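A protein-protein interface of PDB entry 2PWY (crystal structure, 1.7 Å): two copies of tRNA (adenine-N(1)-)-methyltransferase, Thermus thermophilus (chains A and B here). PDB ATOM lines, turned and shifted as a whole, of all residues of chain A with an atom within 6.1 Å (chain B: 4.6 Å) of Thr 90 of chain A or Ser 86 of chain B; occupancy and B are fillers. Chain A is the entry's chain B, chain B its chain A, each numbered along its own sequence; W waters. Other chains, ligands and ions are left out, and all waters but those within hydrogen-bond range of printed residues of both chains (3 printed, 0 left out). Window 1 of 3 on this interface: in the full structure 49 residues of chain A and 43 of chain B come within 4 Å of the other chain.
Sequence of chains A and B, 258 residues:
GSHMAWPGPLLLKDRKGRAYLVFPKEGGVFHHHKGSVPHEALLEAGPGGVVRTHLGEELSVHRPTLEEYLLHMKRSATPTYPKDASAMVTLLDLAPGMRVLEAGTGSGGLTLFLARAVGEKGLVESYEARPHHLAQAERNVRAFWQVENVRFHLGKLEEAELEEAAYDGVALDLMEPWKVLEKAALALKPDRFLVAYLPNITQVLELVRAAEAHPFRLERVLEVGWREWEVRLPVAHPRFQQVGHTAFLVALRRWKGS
Ser 86 of chain A touches its own counterpart, Ser 86 of chain B. Ser 86 of chain A touches Thr 90 of chain B, and with the chains exchanged Thr 90 of chain A touches Ser 86 of chain B. Ala 87 of chain A touches Trp 226 of chain B, and with the chains exchanged Trp 226 of chain A touches Ala 87 of chain B. Thr 90 of chain A touches Trp 226 of chain B, and with the chains exchanged Trp 226 of chain A touches Thr 90 of chain B. 7 positions are printed for both chains.
Thr 90 of chain A touches just these residues of chain B: Ser 86, Phe 113 and Trp 226. Of chain A, only Ser 86 and Thr 90 come within 4 Å of Ser 86 of chain B. Printed residues of chain A within 4 Å of Trp 226 of chain B: Ala 87 (3.6 Å) and Thr 90 (3.98 Å). Of the printed residues of chain B, Ser 86 of chain A touches Ser 86 and Thr 90. The nearest printed residue of chain B that does not touch Thr 90 of chain A is Pro 82 of chain B (4.9 Å).
Water W3 lies within hydrogen-bond range of the side-chain hydroxyl (OG) of Ser 86 of chain B, the side-chain hydroxyl (OG) of Ser 86 of chain A and the backbone NH (N) of Ala 87 of chain B. Water W1 bridges NE1 of Trp 226 of chain A (2.8 Å) and NE1 of Trp 226 of chain B (3.1 Å). Water W2 bridges the backbone carbonyl oxygen (O) of Ser 86 of chain A (3.0 Å) and the side-chain hydroxyl (OG) of Ser 86 of chain B (3.2 Å).
Printed residues of chain A that touch a printed residue of chain B: Ser 86, Ala 87, Thr 90 and Trp 226. Hydrophobic or aromatic side chains of chain A that line the printed part of chain B: Ala 87 and Trp 226. Hydrophobic or aromatic side chains of chain B that line the printed part of chain A: Ala 87, Phe 113 and Trp 226. Among the printed residues, 8 pairs touch across the chains.
OG of Ser 86 of chain A is in hydrogen-bond range of O of Ser 86 of chain B, 3.2 Å away. OG of Ser 86 of chain B sits at hydrogen-bond distance from OG1 of Thr 90 of chain A. The side-chain hydroxyl (OG) of Ser 86 of chain A sits at hydrogen-bond distance from the side-chain hydroxyl (OG1) of Thr 90 of chain B (2.8 Å).
Trp 226 of chain B touches Ala 87 of chain A. OG1 of Thr 90 of chain A touches CE2 of Phe 113 of chain B, at 3.9 Å. CG2 of Thr 90 of chain A touches CH2 of Trp 226 of chain B (3.98 Å). Ala 87 of chain B touches Trp 226 of chain A (CB to CZ2, 3.7 Å). CH2 of Trp 226 of chain A touches CG2 of Thr 90 of chain B (3.99 Å).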
ATOM      1  N   ALA A  85     -11.497   2.122 -13.125  1.00  0.00           N
ATOM      2  CA  ALA A  85     -12.000   2.913 -14.248  1.00  0.00           C
ATOM      3  C   ALA A  85     -11.601   4.374 -14.029  1.00  0.00           C
ATOM      4  O   ALA A  85     -11.149   5.048 -14.965  1.00  0.00           O
ATOM      5  CB  ALA A  85     -13.499   2.760 -14.397  1.00  0.00           C
ATOM      6  N   SER A  86     -11.719   4.821 -12.776  1.00  0.00           N
ATOM      7  CA  SER A  86     -11.320   6.167 -12.346  1.00  0.00           C
ATOM      8  C   SER A  86      -9.832   6.440 -12.690  1.00  0.00           C
ATOM      9  O   SER A  86      -9.491   7.448 -13.345  1.00  0.00           O
ATOM     10  CB  SER A  86     -11.601   6.332 -10.833  1.00  0.00           C
ATOM     11  OG  SER A  86     -11.268   7.647 -10.389  1.00  0.00           O
ATOM     12  N   ALA A  87      -8.954   5.531 -12.269  1.00  0.00           N
ATOM     13  CA  ALA A  87      -7.523   5.666 -12.557  1.00  0.00           C
ATOM     14  C   ALA A  87      -7.251   5.603 -14.054  1.00  0.00           C
ATOM     15  O   ALA A  87      -6.391   6.322 -14.559  1.00  0.00           O
ATOM     16  CB  ALA A  87      -6.730   4.599 -11.831  1.00  0.00           C
ATOM     17  N   MET A  88      -7.956   4.718 -14.764  1.00  0.00           N
ATOM     18  CA  MET A  88      -7.754   4.576 -16.217  1.00  0.00           C
ATOM     19  C   MET A  88      -8.021   5.868 -16.980  1.00  0.00           C
ATOM     20  O   MET A  88      -7.252   6.258 -17.854  1.00  0.00           O
ATOM     21  CB  MET A  88      -8.602   3.430 -16.775  1.00  0.00           C
ATOM     22  CG  MET A  88      -8.057   2.053 -16.391  1.00  0.00           C
ATOM     23  SD  MET A  88      -9.004   0.698 -17.093  1.00  0.00           S
ATOM     24  CE  MET A  88      -8.467   0.738 -18.798  1.00  0.00           C
ATOM     25  N   VAL A  89      -9.101   6.551 -16.626  1.00  0.00           N
ATOM     26  CA  VAL A  89      -9.416   7.846 -17.229  1.00  0.00           C
ATOM     27  C   VAL A  89      -8.282   8.861 -17.008  1.00  0.00           C
ATOM     28  O   VAL A  89      -7.891   9.589 -17.913  1.00  0.00           O
ATOM     29  CB  VAL A  89     -10.774   8.340 -16.688  1.00  0.00           C
ATOM     30  CG1 VAL A  89     -10.997   9.836 -16.971  1.00  0.00           C
ATOM     31  CG2 VAL A  89     -11.905   7.462 -17.252  1.00  0.00           C
ATOM     32  N   THR A  90      -7.709   8.862 -15.810  1.00  0.00           N
ATOM     33  CA  THR A  90      -6.583   9.737 -15.518  1.00  0.00           C
ATOM     34  C   THR A  90      -5.315   9.335 -16.282  1.00  0.00           C
ATOM     35  O   THR A  90      -4.629  10.199 -16.832  1.00  0.00           O
ATOM     36  CB  THR A  90      -6.321   9.831 -14.005  1.00  0.00           C
ATOM     37  OG1 THR A  90      -7.486  10.386 -13.371  1.00  0.00           O
ATOM     38  CG2 THR A  90      -5.126  10.748 -13.723  1.00  0.00           C
ATOM     39  N   LEU A  91      -5.020   8.034 -16.327  1.00  0.00           N
ATOM     40  CA  LEU A  91      -3.819   7.538 -17.034  1.00  0.00           C
ATOM     41  C   LEU A  91      -3.922   7.737 -18.550  1.00  0.00           C
ATOM     42  O   LEU A  91      -2.913   7.953 -19.229  1.00  0.00           O
ATOM     43  CB  LEU A  91      -3.554   6.063 -16.710  1.00  0.00           C
ATOM     44  CG  LEU A  91      -3.160   5.788 -15.244  1.00  0.00           C
ATOM     45  CD1 LEU A  91      -3.231   4.301 -14.950  1.00  0.00           C
ATOM     46  CD2 LEU A  91      -1.774   6.350 -14.939  1.00  0.00           C
ATOM     47  N   LEU A  92      -5.141   7.659 -19.065  1.00  0.00           N
ATOM     48  CA  LEU A  92      -5.445   7.974 -20.468  1.00  0.00           C
ATOM     49  C   LEU A  92      -5.438   9.481 -20.730  1.00  0.00           C
ATOM     50  O   LEU A  92      -5.451   9.923 -21.897  1.00  0.00           O
ATOM     51  CB  LEU A  92      -6.814   7.405 -20.832  1.00  0.00           C
ATOM     52  CG  LEU A  92      -6.871   5.890 -21.040  1.00  0.00           C
ATOM     53  CD1 LEU A  92      -8.323   5.379 -20.977  1.00  0.00           C
ATOM     54  CD2 LEU A  92      -6.175   5.517 -22.360  1.00  0.00           C
ATOM     55  N   ASP A  93      -5.421  10.262 -19.649  1.00  0.00           N
ATOM     56  CA  ASP A  93      -5.381  11.725 -19.718  1.00  0.00           C
ATOM     57  C   ASP A  93      -6.538  12.276 -20.563  1.00  0.00           C
ATOM     58  O   ASP A  93      -6.323  13.113 -21.441  1.00  0.00           O
ATOM     59  CB  ASP A  93      -4.006  12.207 -20.269  1.00  0.00           C
ATOM     60  CG  ASP A  93      -3.824  13.711 -20.178  1.00  0.00           C
ATOM     61  OD1 ASP A  93      -4.219  14.305 -19.139  1.00  0.00           O
ATOM     62  OD2 ASP A  93      -3.293  14.292 -21.158  1.00  0.00           O
ATOM     63  N   LEU A  94      -7.755  11.799 -20.296  1.00  0.00           N
ATOM     64  CA  LEU A  94      -8.910  12.182 -21.112  1.00  0.00           C
ATOM     65  C   LEU A  94      -9.464  13.531 -20.673  1.00  0.00           C
ATOM     66  O   LEU A  94      -9.766  13.730 -19.497  1.00  0.00           O
ATOM     67  CB  LEU A  94     -10.006  11.108 -21.069  1.00  0.00           C
ATOM     68  CG  LEU A  94      -9.604   9.754 -21.677  1.00  0.00           C
ATOM     69  CD1 LEU A  94     -10.758   8.770 -21.589  1.00  0.00           C
ATOM     70  CD2 LEU A  94      -9.098   9.881 -23.129  1.00  0.00           C
ATOM     71  N   TRP A 226      -8.215   1.229  -3.043  1.00  0.00           N
ATOM     72  CA  TRP A 226      -9.025   2.174  -2.278  1.00  0.00           C
ATOM     73  C   TRP A 226      -9.337   1.480  -0.969  1.00  0.00           C
ATOM     74  O   TRP A 226     -10.228   0.622  -0.892  1.00  0.00           O
ATOM     75  CB  TRP A 226     -10.319   2.543  -3.013  1.00  0.00           C
ATOM     76  CG  TRP A 226     -10.167   3.530  -4.145  1.00  0.00           C
ATOM     77  CD1 TRP A 226      -8.999   3.959  -4.735  1.00  0.00           C
ATOM     78  CD2 TRP A 226     -11.230   4.177  -4.847  1.00  0.00           C
ATOM     79  NE1 TRP A 226      -9.284   4.845  -5.754  1.00  0.00           N
ATOM     80  CE2 TRP A 226     -10.645   4.994  -5.842  1.00  0.00           C
ATOM     81  CE3 TRP A 226     -12.628   4.152  -4.730  1.00  0.00           C
ATOM     82  CZ2 TRP A 226     -11.411   5.789  -6.713  1.00  0.00           C
ATOM     83  CZ3 TRP A 226     -13.398   4.951  -5.611  1.00  0.00           C
ATOM     84  CH2 TRP A 226     -12.782   5.748  -6.584  1.00  0.00           C
ATOM     85  N   PRO B  82      -2.309  13.615  -7.909  1.00  0.00           N
ATOM     86  CA  PRO B  82      -3.158  13.059  -8.967  1.00  0.00           C
ATOM     87  C   PRO B  82      -4.005  11.839  -8.578  1.00  0.00           C
ATOM     88  O   PRO B  82      -5.169  11.794  -8.924  1.00  0.00           O
ATOM     89  CB  PRO B  82      -2.143  12.728 -10.075  1.00  0.00           C
ATOM     90  CG  PRO B  82      -1.117  13.770  -9.905  1.00  0.00           C
ATOM     91  CD  PRO B  82      -0.932  13.820  -8.401  1.00  0.00           C
ATOM     92  N   LYS B  83      -3.459  10.877  -7.837  1.00  0.00           N
ATOM     93  CA  LYS B  83      -4.255   9.702  -7.462  1.00  0.00           C
ATOM     94  C   LYS B  83      -5.482  10.109  -6.634  1.00  0.00           C
ATOM     95  O   LYS B  83      -6.565   9.508  -6.724  1.00  0.00           O
ATOM     96  CB  LYS B  83      -3.397   8.691  -6.695  1.00  0.00           C
ATOM     97  CG  LYS B  83      -2.947   9.148  -5.311  1.00  0.00           C
ATOM     98  CD  LYS B  83      -2.108   8.078  -4.620  1.00  0.00           C
ATOM     99  CE  LYS B  83      -1.658   8.587  -3.240  1.00  0.00           C
ATOM    100  NZ  LYS B  83      -2.785   8.758  -2.269  1.00  0.00           N
ATOM    101  N   ASP B  84      -5.292  11.130  -5.807  1.00  0.00           N
ATOM    102  CA  ASP B  84      -6.346  11.594  -4.910  1.00  0.00           C
ATOM    103  C   ASP B  84      -7.356  12.470  -5.632  1.00  0.00           C
ATOM    104  O   ASP B  84      -8.556  12.351  -5.389  1.00  0.00           O
ATOM    105  CB  ASP B  84      -5.720  12.345  -3.732  1.00  0.00           C
ATOM    106  CG  ASP B  84      -4.715  11.484  -2.967  1.00  0.00           C
ATOM    107  OD1 ASP B  84      -5.079  10.349  -2.626  1.00  0.00           O
ATOM    108  OD2 ASP B  84      -3.576  11.938  -2.745  1.00  0.00           O
ATOM    109  N   ALA B  85      -6.879  13.343  -6.515  1.00  0.00           N
ATOM    110  CA  ALA B  85      -7.773  14.230  -7.277  1.00  0.00           C
ATOM    111  C   ALA B  85      -8.674  13.392  -8.193  1.00  0.00           C
ATOM    112  O   ALA B  85      -9.880  13.628  -8.282  1.00  0.00           O
ATOM    113  CB  ALA B  85      -6.974  15.250  -8.066  1.00  0.00           C
ATOM    114  N   SER B  86      -8.078  12.393  -8.833  1.00  0.00           N
ATOM    115  CA  SER B  86      -8.802  11.412  -9.638  1.00  0.00           C
ATOM    116  C   SER B  86      -9.924  10.732  -8.837  1.00  0.00           C
ATOM    117  O   SER B  86     -11.082  10.665  -9.290  1.00  0.00           O
ATOM    118  CB  SER B  86      -7.798  10.366 -10.152  1.00  0.00           C
ATOM    119  OG  SER B  86      -8.437   9.374 -10.933  1.00  0.00           O
ATOM    120  N   ALA B  87      -9.590  10.233  -7.646  1.00  0.00           N
ATOM    121  CA  ALA B  87     -10.576   9.587  -6.775  1.00  0.00           C
ATOM    122  C   ALA B  87     -11.647  10.566  -6.313  1.00  0.00           C
ATOM    123  O   ALA B  87     -12.832  10.213  -6.257  1.00  0.00           O
ATOM    124  CB  ALA B  87      -9.897   8.919  -5.587  1.00  0.00           C
ATOM    125  N   MET B  88     -11.241  11.794  -5.991  1.00  0.00           N
ATOM    126  CA  MET B  88     -12.215  12.789  -5.517  1.00  0.00           C
ATOM    127  C   MET B  88     -13.292  13.088  -6.551  1.00  0.00           C
ATOM    128  O   MET B  88     -14.463  13.218  -6.205  1.00  0.00           O
ATOM    129  CB  MET B  88     -11.525  14.075  -5.076  1.00  0.00           C
ATOM    130  CG  MET B  88     -10.750  13.895  -3.804  1.00  0.00           C
ATOM    131  SD  MET B  88      -9.875  15.386  -3.327  1.00  0.00           S
ATOM    132  CE  MET B  88     -11.242  16.350  -2.668  1.00  0.00           C
ATOM    133  N   VAL B  89     -12.905  13.171  -7.821  1.00  0.00           N
ATOM    134  CA  VAL B  89     -13.880  13.415  -8.880  1.00  0.00           C
ATOM    135  C   VAL B  89     -14.911  12.286  -8.963  1.00  0.00           C
ATOM    136  O   VAL B  89     -16.106  12.539  -9.151  1.00  0.00           O
ATOM    137  CB  VAL B  89     -13.180  13.651 -10.220  1.00  0.00           C
ATOM    138  CG1 VAL B  89     -14.192  13.646 -11.369  1.00  0.00           C
ATOM    139  CG2 VAL B  89     -12.420  14.988 -10.157  1.00  0.00           C
ATOM    140  N   THR B  90     -14.451  11.047  -8.798  1.00  0.00           N
ATOM    141  CA  THR B  90     -15.348   9.894  -8.817  1.00  0.00           C
ATOM    142  C   THR B  90     -16.227   9.852  -7.564  1.00  0.00           C
ATOM    143  O   THR B  90     -17.424   9.580  -7.642  1.00  0.00           O
ATOM    144  CB  THR B  90     -14.566   8.572  -8.966  1.00  0.00           C
ATOM    145  OG1 THR B  90     -13.867   8.602 -10.222  1.00  0.00           O
ATOM    146  CG2 THR B  90     -15.538   7.371  -8.976  1.00  0.00           C
ATOM    147  N   PHE B 113      -8.615  19.123 -12.310  1.00  0.00           N
ATOM    148  CA  PHE B 113      -9.357  17.857 -12.335  1.00  0.00           C
ATOM    149  C   PHE B 113     -10.867  18.122 -12.320  1.00  0.00           C
ATOM    150  O   PHE B 113     -11.635  17.549 -13.115  1.00  0.00           O
ATOM    151  CB  PHE B 113      -8.951  16.965 -11.156  1.00  0.00           C
ATOM    152  CG  PHE B 113      -7.743  16.118 -11.445  1.00  0.00           C
ATOM    153  CD1 PHE B 113      -6.462  16.653 -11.343  1.00  0.00           C
ATOM    154  CD2 PHE B 113      -7.898  14.790 -11.855  1.00  0.00           C
ATOM    155  CE1 PHE B 113      -5.321  15.863 -11.639  1.00  0.00           C
ATOM    156  CE2 PHE B 113      -6.776  13.997 -12.147  1.00  0.00           C
ATOM    157  CZ  PHE B 113      -5.495  14.533 -12.043  1.00  0.00           C
ATOM    158  N   TRP B 226      -1.745   4.128  -5.283  1.00  0.00           N
ATOM    159  CA  TRP B 226      -1.351   3.692  -6.625  1.00  0.00           C
ATOM    160  C   TRP B 226       0.034   3.086  -6.467  1.00  0.00           C
ATOM    161  O   TRP B 226       1.052   3.800  -6.392  1.00  0.00           O
ATOM    162  CB  TRP B 226      -1.336   4.847  -7.626  1.00  0.00           C
ATOM    163  CG  TRP B 226      -2.698   5.329  -8.109  1.00  0.00           C
ATOM    164  CD1 TRP B 226      -3.927   4.997  -7.612  1.00  0.00           C
ATOM    165  CD2 TRP B 226      -2.933   6.265  -9.173  1.00  0.00           C
ATOM    166  NE1 TRP B 226      -4.918   5.665  -8.313  1.00  0.00           N
ATOM    167  CE2 TRP B 226      -4.330   6.445  -9.275  1.00  0.00           C
ATOM    168  CE3 TRP B 226      -2.091   6.969 -10.050  1.00  0.00           C
ATOM    169  CZ2 TRP B 226      -4.911   7.305 -10.226  1.00  0.00           C
ATOM    170  CZ3 TRP B 226      -2.667   7.816 -11.002  1.00  0.00           C
ATOM    171  CH2 TRP B 226      -4.060   7.977 -11.076  1.00  0.00           C
HETATM  172  O   HOH W   1      -8.044   5.427  -8.142  1.00  0.00           O
HETATM  173  O   HOH W   2     -10.995   9.972 -12.685  1.00  0.00           O
HETATM  174  O   HOH W   3      -8.802   7.430  -9.315  1.00  0.00           O
